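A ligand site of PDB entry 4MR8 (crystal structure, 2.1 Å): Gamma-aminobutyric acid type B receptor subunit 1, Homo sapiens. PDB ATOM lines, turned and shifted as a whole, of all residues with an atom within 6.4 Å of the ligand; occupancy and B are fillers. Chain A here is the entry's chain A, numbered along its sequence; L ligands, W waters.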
ATOM      1  N   GLY A  16     -25.706  -6.497  17.345  1.00  0.00           N
ATOM      2  CA  GLY A  16     -25.022  -6.482  16.058  1.00  0.00           C
ATOM      3  C   GLY A  16     -24.640  -5.091  15.606  1.00  0.00           C
ATOM      4  O   GLY A  16     -24.574  -4.164  16.432  1.00  0.00           O
ATOM      5  N   GLY A  17     -24.384  -4.944  14.303  1.00  0.00           N
ATOM      6  CA  GLY A  17     -23.984  -3.681  13.672  1.00  0.00           C
ATOM      7  C   GLY A  17     -24.979  -2.556  13.833  1.00  0.00           C
ATOM      8  O   GLY A  17     -24.587  -1.402  14.068  1.00  0.00           O
ATOM      9  N   TRP A  18     -26.281  -2.873  13.683  1.00  0.00           N
ATOM     10  CA  TRP A  18     -27.352  -1.908  13.879  1.00  0.00           C
ATOM     11  C   TRP A  18     -28.373  -2.544  14.825  1.00  0.00           C
ATOM     12  O   TRP A  18     -29.216  -3.346  14.390  1.00  0.00           O
ATOM     13  CB  TRP A  18     -28.006  -1.460  12.553  1.00  0.00           C
ATOM     14  CG  TRP A  18     -29.153  -0.503  12.753  1.00  0.00           C
ATOM     15  CD1 TRP A  18     -29.079   0.780  13.195  1.00  0.00           C
ATOM     16  CD2 TRP A  18     -30.547  -0.783  12.530  1.00  0.00           C
ATOM     17  NE1 TRP A  18     -30.340   1.344  13.243  1.00  0.00           N
ATOM     18  CE2 TRP A  18     -31.260   0.409  12.823  1.00  0.00           C
ATOM     19  CE3 TRP A  18     -31.263  -1.907  12.075  1.00  0.00           C
ATOM     20  CZ2 TRP A  18     -32.653   0.498  12.664  1.00  0.00           C
ATOM     21  CZ3 TRP A  18     -32.645  -1.825  11.955  1.00  0.00           C
ATOM     22  CH2 TRP A  18     -33.329  -0.640  12.254  1.00  0.00           C
ATOM     23  N   CYS A  56     -28.606  -8.893  13.874  1.00  0.00           N
ATOM     24  CA  CYS A  56     -28.112  -8.178  12.679  1.00  0.00           C
ATOM     25  C   CYS A  56     -27.077  -9.054  11.910  1.00  0.00           C
ATOM     26  O   CYS A  56     -26.090  -8.552  11.373  1.00  0.00           O
ATOM     27  CB  CYS A  56     -27.530  -6.818  13.088  1.00  0.00           C
ATOM     28  SG  CYS A  56     -27.413  -5.609  11.748  1.00  0.00           S
ATOM     29  N   GLY A  81     -35.069  -6.143   9.642  1.00  0.00           N
ATOM     30  CA  GLY A  81     -34.514  -4.837   9.974  1.00  0.00           C
ATOM     31  C   GLY A  81     -33.287  -4.427   9.188  1.00  0.00           C
ATOM     32  O   GLY A  81     -33.386  -3.577   8.320  1.00  0.00           O
ATOM     33  N   CYS A  82     -32.114  -5.017   9.529  1.00  0.00           N
ATOM     34  CA  CYS A  82     -30.788  -4.788   8.920  1.00  0.00           C
ATOM     35  C   CYS A  82     -30.801  -5.057   7.429  1.00  0.00           C
ATOM     36  O   CYS A  82     -31.568  -5.919   6.965  1.00  0.00           O
ATOM     37  CB  CYS A  82     -29.718  -5.617   9.632  1.00  0.00           C
ATOM     38  SG  CYS A  82     -29.314  -5.003  11.294  1.00  0.00           S
ATOM     39  N   SER A  83     -29.931  -4.350   6.685  1.00  0.00           N
ATOM     40  CA  SER A  83     -29.747  -4.495   5.243  1.00  0.00           C
ATOM     41  C   SER A  83     -29.266  -5.912   4.903  1.00  0.00           C
ATOM     42  O   SER A  83     -29.824  -6.524   4.028  1.00  0.00           O
ATOM     43  CB  SER A  83     -28.769  -3.453   4.711  1.00  0.00           C
ATOM     44  OG  SER A  83     -29.438  -2.216   4.547  1.00  0.00           O
ATOM     45  N   SER A  84     -28.290  -6.438   5.658  1.00  0.00           N
ATOM     46  CA  SER A  84     -27.723  -7.773   5.450  1.00  0.00           C
ATOM     47  C   SER A  84     -28.790  -8.861   5.655  1.00  0.00           C
ATOM     48  O   SER A  84     -28.841  -9.834   4.904  1.00  0.00           O
ATOM     49  CB  SER A  84     -26.524  -8.009   6.363  1.00  0.00           C
ATOM     50  OG  SER A  84     -26.905  -8.048   7.735  1.00  0.00           O
ATOM     51  N   GLY A 104     -35.772  -0.890   8.526  1.00  0.00           N
ATOM     52  CA  GLY A 104     -34.449  -0.309   8.775  1.00  0.00           C
ATOM     53  C   GLY A 104     -33.369  -0.417   7.706  1.00  0.00           C
ATOM     54  O   GLY A 104     -32.254  -0.001   7.960  1.00  0.00           O
ATOM     55  N   SER A 105     -33.685  -0.946   6.517  1.00  0.00           N
ATOM     56  CA  SER A 105     -32.654  -1.147   5.477  1.00  0.00           C
ATOM     57  C   SER A 105     -32.373   0.059   4.602  1.00  0.00           C
ATOM     58  O   SER A 105     -33.294   0.580   3.981  1.00  0.00           O
ATOM     59  CB  SER A 105     -32.966  -2.372   4.635  1.00  0.00           C
ATOM     60  OG  SER A 105     -32.983  -3.511   5.479  1.00  0.00           O
ATOM     61  N   SER A 106     -31.105   0.502   4.558  1.00  0.00           N
ATOM     62  CA  SER A 106     -30.675   1.665   3.774  1.00  0.00           C
ATOM     63  C   SER A 106     -29.834   1.328   2.534  1.00  0.00           C
ATOM     64  O   SER A 106     -29.597   2.212   1.704  1.00  0.00           O
ATOM     65  CB  SER A 106     -29.852   2.598   4.649  1.00  0.00           C
ATOM     66  OG  SER A 106     -28.615   1.986   5.012  1.00  0.00           O
ATOM     67  N   SER A 107     -29.351   0.069   2.415  1.00  0.00           N
ATOM     68  CA  SER A 107     -28.483  -0.339   1.316  1.00  0.00           C
ATOM     69  C   SER A 107     -29.074  -0.093  -0.083  1.00  0.00           C
ATOM     70  O   SER A 107     -30.150  -0.604  -0.380  1.00  0.00           O
ATOM     71  CB  SER A 107     -28.040  -1.791   1.469  1.00  0.00           C
ATOM     72  OG  SER A 107     -27.204  -2.180   0.397  1.00  0.00           O
ATOM     73  N   PRO A 108     -28.362   0.669  -0.964  1.00  0.00           N
ATOM     74  CA  PRO A 108     -28.906   0.938  -2.315  1.00  0.00           C
ATOM     75  C   PRO A 108     -29.209  -0.296  -3.161  1.00  0.00           C
ATOM     76  O   PRO A 108     -30.133  -0.277  -3.984  1.00  0.00           O
ATOM     77  CB  PRO A 108     -27.829   1.817  -2.957  1.00  0.00           C
ATOM     78  CG  PRO A 108     -27.141   2.490  -1.779  1.00  0.00           C
ATOM     79  CD  PRO A 108     -27.093   1.400  -0.742  1.00  0.00           C
ATOM     80  N   HIS A 123     -37.790   2.602   5.292  1.00  0.00           N
ATOM     81  CA  HIS A 123     -36.506   3.258   5.463  1.00  0.00           C
ATOM     82  C   HIS A 123     -36.028   3.584   4.053  1.00  0.00           C
ATOM     83  O   HIS A 123     -35.945   2.670   3.228  1.00  0.00           O
ATOM     84  CB  HIS A 123     -35.477   2.344   6.174  1.00  0.00           C
ATOM     85  CG  HIS A 123     -34.189   3.042   6.521  1.00  0.00           C
ATOM     86  ND1 HIS A 123     -33.251   3.324   5.568  1.00  0.00           N
ATOM     87  CD2 HIS A 123     -33.724   3.460   7.724  1.00  0.00           C
ATOM     88  CE1 HIS A 123     -32.262   3.933   6.190  1.00  0.00           C
ATOM     89  NE2 HIS A 123     -32.488   4.007   7.498  1.00  0.00           N
ATOM     90  N   THR A 152     -16.685   0.613   1.252  1.00  0.00           N
ATOM     91  CA  THR A 152     -17.777  -0.165   1.831  1.00  0.00           C
ATOM     92  C   THR A 152     -18.749  -0.230   0.694  1.00  0.00           C
ATOM     93  O   THR A 152     -18.819   0.717  -0.104  1.00  0.00           O
ATOM     94  CB  THR A 152     -18.394   0.485   3.102  1.00  0.00           C
ATOM     95  OG1 THR A 152     -17.375   0.981   3.952  1.00  0.00           O
ATOM     96  CG2 THR A 152     -19.245  -0.501   3.894  1.00  0.00           C
ATOM     97  N   VAL A 154     -21.986  -0.008   0.575  1.00  0.00           N
ATOM     98  CA  VAL A 154     -22.967   1.077   0.673  1.00  0.00           C
ATOM     99  C   VAL A 154     -22.489   2.392   0.031  1.00  0.00           C
ATOM    100  O   VAL A 154     -23.258   3.013  -0.703  1.00  0.00           O
ATOM    101  CB  VAL A 154     -23.540   1.265   2.113  1.00  0.00           C
ATOM    102  CG1 VAL A 154     -22.444   1.614   3.131  1.00  0.00           C
ATOM    103  CG2 VAL A 154     -24.669   2.285   2.145  1.00  0.00           C
ATOM    104  N   TYR A 203     -17.723   6.470   7.545  1.00  0.00           N
ATOM    105  CA  TYR A 203     -18.212   6.369   8.909  1.00  0.00           C
ATOM    106  C   TYR A 203     -17.446   7.350   9.811  1.00  0.00           C
ATOM    107  O   TYR A 203     -16.503   8.006   9.357  1.00  0.00           O
ATOM    108  CB  TYR A 203     -18.124   4.927   9.414  1.00  0.00           C
ATOM    109  CG  TYR A 203     -19.129   4.029   8.741  1.00  0.00           C
ATOM    110  CD1 TYR A 203     -20.500   4.193   8.959  1.00  0.00           C
ATOM    111  CD2 TYR A 203     -18.729   3.006   7.880  1.00  0.00           C
ATOM    112  CE1 TYR A 203     -21.440   3.377   8.320  1.00  0.00           C
ATOM    113  CE2 TYR A 203     -19.649   2.186   7.245  1.00  0.00           C
ATOM    114  CZ  TYR A 203     -21.003   2.382   7.468  1.00  0.00           C
ATOM    115  OH  TYR A 203     -21.932   1.580   6.843  1.00  0.00           O
ATOM    116  N   TRP A 231     -25.025  11.981   9.818  1.00  0.00           N
ATOM    117  CA  TRP A 231     -25.334  10.859  10.718  1.00  0.00           C
ATOM    118  C   TRP A 231     -24.308  10.712  11.863  1.00  0.00           C
ATOM    119  O   TRP A 231     -24.333   9.709  12.596  1.00  0.00           O
ATOM    120  CB  TRP A 231     -25.454   9.544   9.909  1.00  0.00           C
ATOM    121  CG  TRP A 231     -24.206   9.108   9.170  1.00  0.00           C
ATOM    122  CD1 TRP A 231     -22.985   9.720   9.142  1.00  0.00           C
ATOM    123  CD2 TRP A 231     -24.093   7.931   8.357  1.00  0.00           C
ATOM    124  NE1 TRP A 231     -22.110   9.002   8.363  1.00  0.00           N
ATOM    125  CE2 TRP A 231     -22.764   7.886   7.873  1.00  0.00           C
ATOM    126  CE3 TRP A 231     -24.975   6.897   7.996  1.00  0.00           C
ATOM    127  CZ2 TRP A 231     -22.305   6.865   7.036  1.00  0.00           C
ATOM    128  CZ3 TRP A 231     -24.518   5.887   7.179  1.00  0.00           C
ATOM    129  CH2 TRP A 231     -23.200   5.882   6.694  1.00  0.00           C
ATOM    130  N   MET A 265     -36.587  11.317   9.482  1.00  0.00           N
ATOM    131  CA  MET A 265     -37.211  10.112  10.044  1.00  0.00           C
ATOM    132  C   MET A 265     -38.404  10.408  10.961  1.00  0.00           C
ATOM    133  O   MET A 265     -39.115   9.478  11.354  1.00  0.00           O
ATOM    134  CB  MET A 265     -36.170   9.255  10.762  1.00  0.00           C
ATOM    135  CG  MET A 265     -35.181   8.605   9.817  1.00  0.00           C
ATOM    136  SD  MET A 265     -34.058   7.508  10.676  1.00  0.00           S
ATOM    137  CE  MET A 265     -32.774   7.347   9.477  1.00  0.00           C
ATOM    138  N   GLN A 301     -34.137   6.563  16.623  1.00  0.00           N
ATOM    139  CA  GLN A 301     -34.410   7.498  15.530  1.00  0.00           C
ATOM    140  C   GLN A 301     -35.123   6.837  14.338  1.00  0.00           C
ATOM    141  O   GLN A 301     -35.850   7.516  13.622  1.00  0.00           O
ATOM    142  CB  GLN A 301     -33.151   8.265  15.097  1.00  0.00           C
ATOM    143  CG  GLN A 301     -32.027   7.402  14.515  1.00  0.00           C
ATOM    144  CD  GLN A 301     -31.050   8.200  13.659  1.00  0.00           C
ATOM    145  OE1 GLN A 301     -31.232   9.391  13.375  1.00  0.00           O
ATOM    146  NE2 GLN A 301     -30.004   7.520  13.208  1.00  0.00           N
ATOM    147  N   GLU A 302     -34.938   5.509  14.158  1.00  0.00           N
ATOM    148  CA  GLU A 302     -35.573   4.726  13.101  1.00  0.00           C
ATOM    149  C   GLU A 302     -36.947   4.208  13.516  1.00  0.00           C
ATOM    150  O   GLU A 302     -37.717   3.778  12.655  1.00  0.00           O
ATOM    151  CB  GLU A 302     -34.672   3.572  12.608  1.00  0.00           C
ATOM    152  CG  GLU A 302     -33.481   4.016  11.781  1.00  0.00           C
ATOM    153  CD  GLU A 302     -32.247   4.417  12.552  1.00  0.00           C
ATOM    154  OE1 GLU A 302     -32.154   4.065  13.759  1.00  0.00           O
ATOM    155  OE2 GLU A 302     -31.359   5.071  11.958  1.00  0.00           O
ATOM    156  N   LEU A 305     -40.232   4.755  11.497  1.00  0.00           N
ATOM    157  CA  LEU A 305     -40.290   3.983  10.254  1.00  0.00           C
ATOM    158  C   LEU A 305     -40.889   2.602  10.501  1.00  0.00           C
ATOM    159  O   LEU A 305     -41.623   2.112   9.648  1.00  0.00           O
ATOM    160  CB  LEU A 305     -38.901   3.849   9.584  1.00  0.00           C
ATOM    161  CG  LEU A 305     -38.070   5.128   9.417  1.00  0.00           C
ATOM    162  CD1 LEU A 305     -36.640   4.805   9.039  1.00  0.00           C
ATOM    163  CD2 LEU A 305     -38.701   6.086   8.411  1.00  0.00           C
HETATM  164  O1  LIG L   1     -28.531  -2.393   7.914  1.00  0.00           O
HETATM  165  P1  LIG L   1     -28.439  -0.917   7.791  1.00  0.00           P
HETATM  166  O2  LIG L   1     -29.001  -0.430   6.372  1.00  0.00           O
HETATM  167  C1  LIG L   1     -29.342  -0.159   9.147  1.00  0.00           C
HETATM  168  C2  LIG L   1     -29.363   1.354   8.955  1.00  0.00           C
HETATM  169  C3  LIG L   1     -30.355   1.963   9.920  1.00  0.00           C
HETATM  170  N1  LIG L   1     -30.550   3.364   9.578  1.00  0.00           N
HETATM  171  C4  LIG L   1     -26.728  -0.324   8.002  1.00  0.00           C
HETATM  172  O3  LIG L   1     -25.990  -1.230   8.814  1.00  0.00           O
HETATM  173  C5  LIG L   1     -24.947  -0.618   9.577  1.00  0.00           C
HETATM  174  C6  LIG L   1     -24.368  -1.704  10.442  1.00  0.00           C
HETATM  175  O4  LIG L   1     -26.062  -0.078   6.761  1.00  0.00           O
HETATM  176  C7  LIG L   1     -25.760  -1.256   5.995  1.00  0.00           C
HETATM  177  C8  LIG L   1     -25.577  -0.879   4.548  1.00  0.00           C
HETATM  178  O   HOH W   1     -24.669   2.243   6.890  1.00  0.00           O
HETATM  179  O   HOH W   2     -26.779  -4.622   7.750  1.00  0.00           O
HETATM  180  O   HOH W   3     -26.855   1.769  11.112  1.00  0.00           O
HETATM  181  O   HOH W   4     -27.939   4.769   8.823  1.00  0.00           O
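Merely in contact with the ligand: Gly 17 (3.5 Å), Trp 18 (3.4 Å), Cys 82 (3.4 Å), Gly 104 (3.1 Å), Ser 105 (3.8 Å) and Val 154 (3.8 Å).
Hydrophobic or aromatic side chains that line the ligand: Trp 18, His 123 and Val 154.
SG of Cys 56 is disulfide-bonded to SG of Cys 82 (2.0 Å).
The side-chain hydroxyl (OG) of Ser 105 lies within hydrogen-bond range of the backbone carbonyl oxygen (O) of Gly 81 (2.9 Å).
OG of Ser 83 is in hydrogen-bond range of N of Ser 107 (3.1 Å).
N of Trp 18 is in hydrogen-bond range of SG of Cys 56 (3.5 Å).
OG of Ser 83 is in hydrogen-bond range of N of Ser 106.
The side-chain carboxylate (OE2) of Glu 302 lies within hydrogen-bond range of the side-chain amide nitrogen (NE2) of Gln 301 (3.1 Å).
The side-chain hydroxyl of Ser 105 lies within hydrogen-bond range of the backbone carbonyl oxygen of Cys 82 (3.2 Å).
A ring nitrogen (ND1) of His 123 is in hydrogen-bond range of the backbone carbonyl oxygen of Ser 105.
NE2 of His 123 is in hydrogen-bond range of N1 of the ligand (2.9 Å).
The side-chain carboxylate (OE2) of Glu 302 is in salt-bridge range of a nitrogen (N1) of the ligand (3.0 Å).
An oxygen (O2) of the ligand is in hydrogen-bond range of the backbone NH of Ser 106, at 2.9 Å.
O2 of the ligand sits at hydrogen-bond distance from OG of Ser 83.
N of Ser 83 is in hydrogen-bond range of O1 of the ligand, 2.7 Å away.
OG of Ser 106 lies within hydrogen-bond range of O2 of the ligand.
Water W1 bridges O4 of the ligand (2.7 Å) and OH of Tyr 203 (2.8 Å).
Water W2 lies within hydrogen-bond range of O1 of the ligand (2.8 Å), N of Ser 84 (3.2 Å) and N of Ser 83 (3.3 Å).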
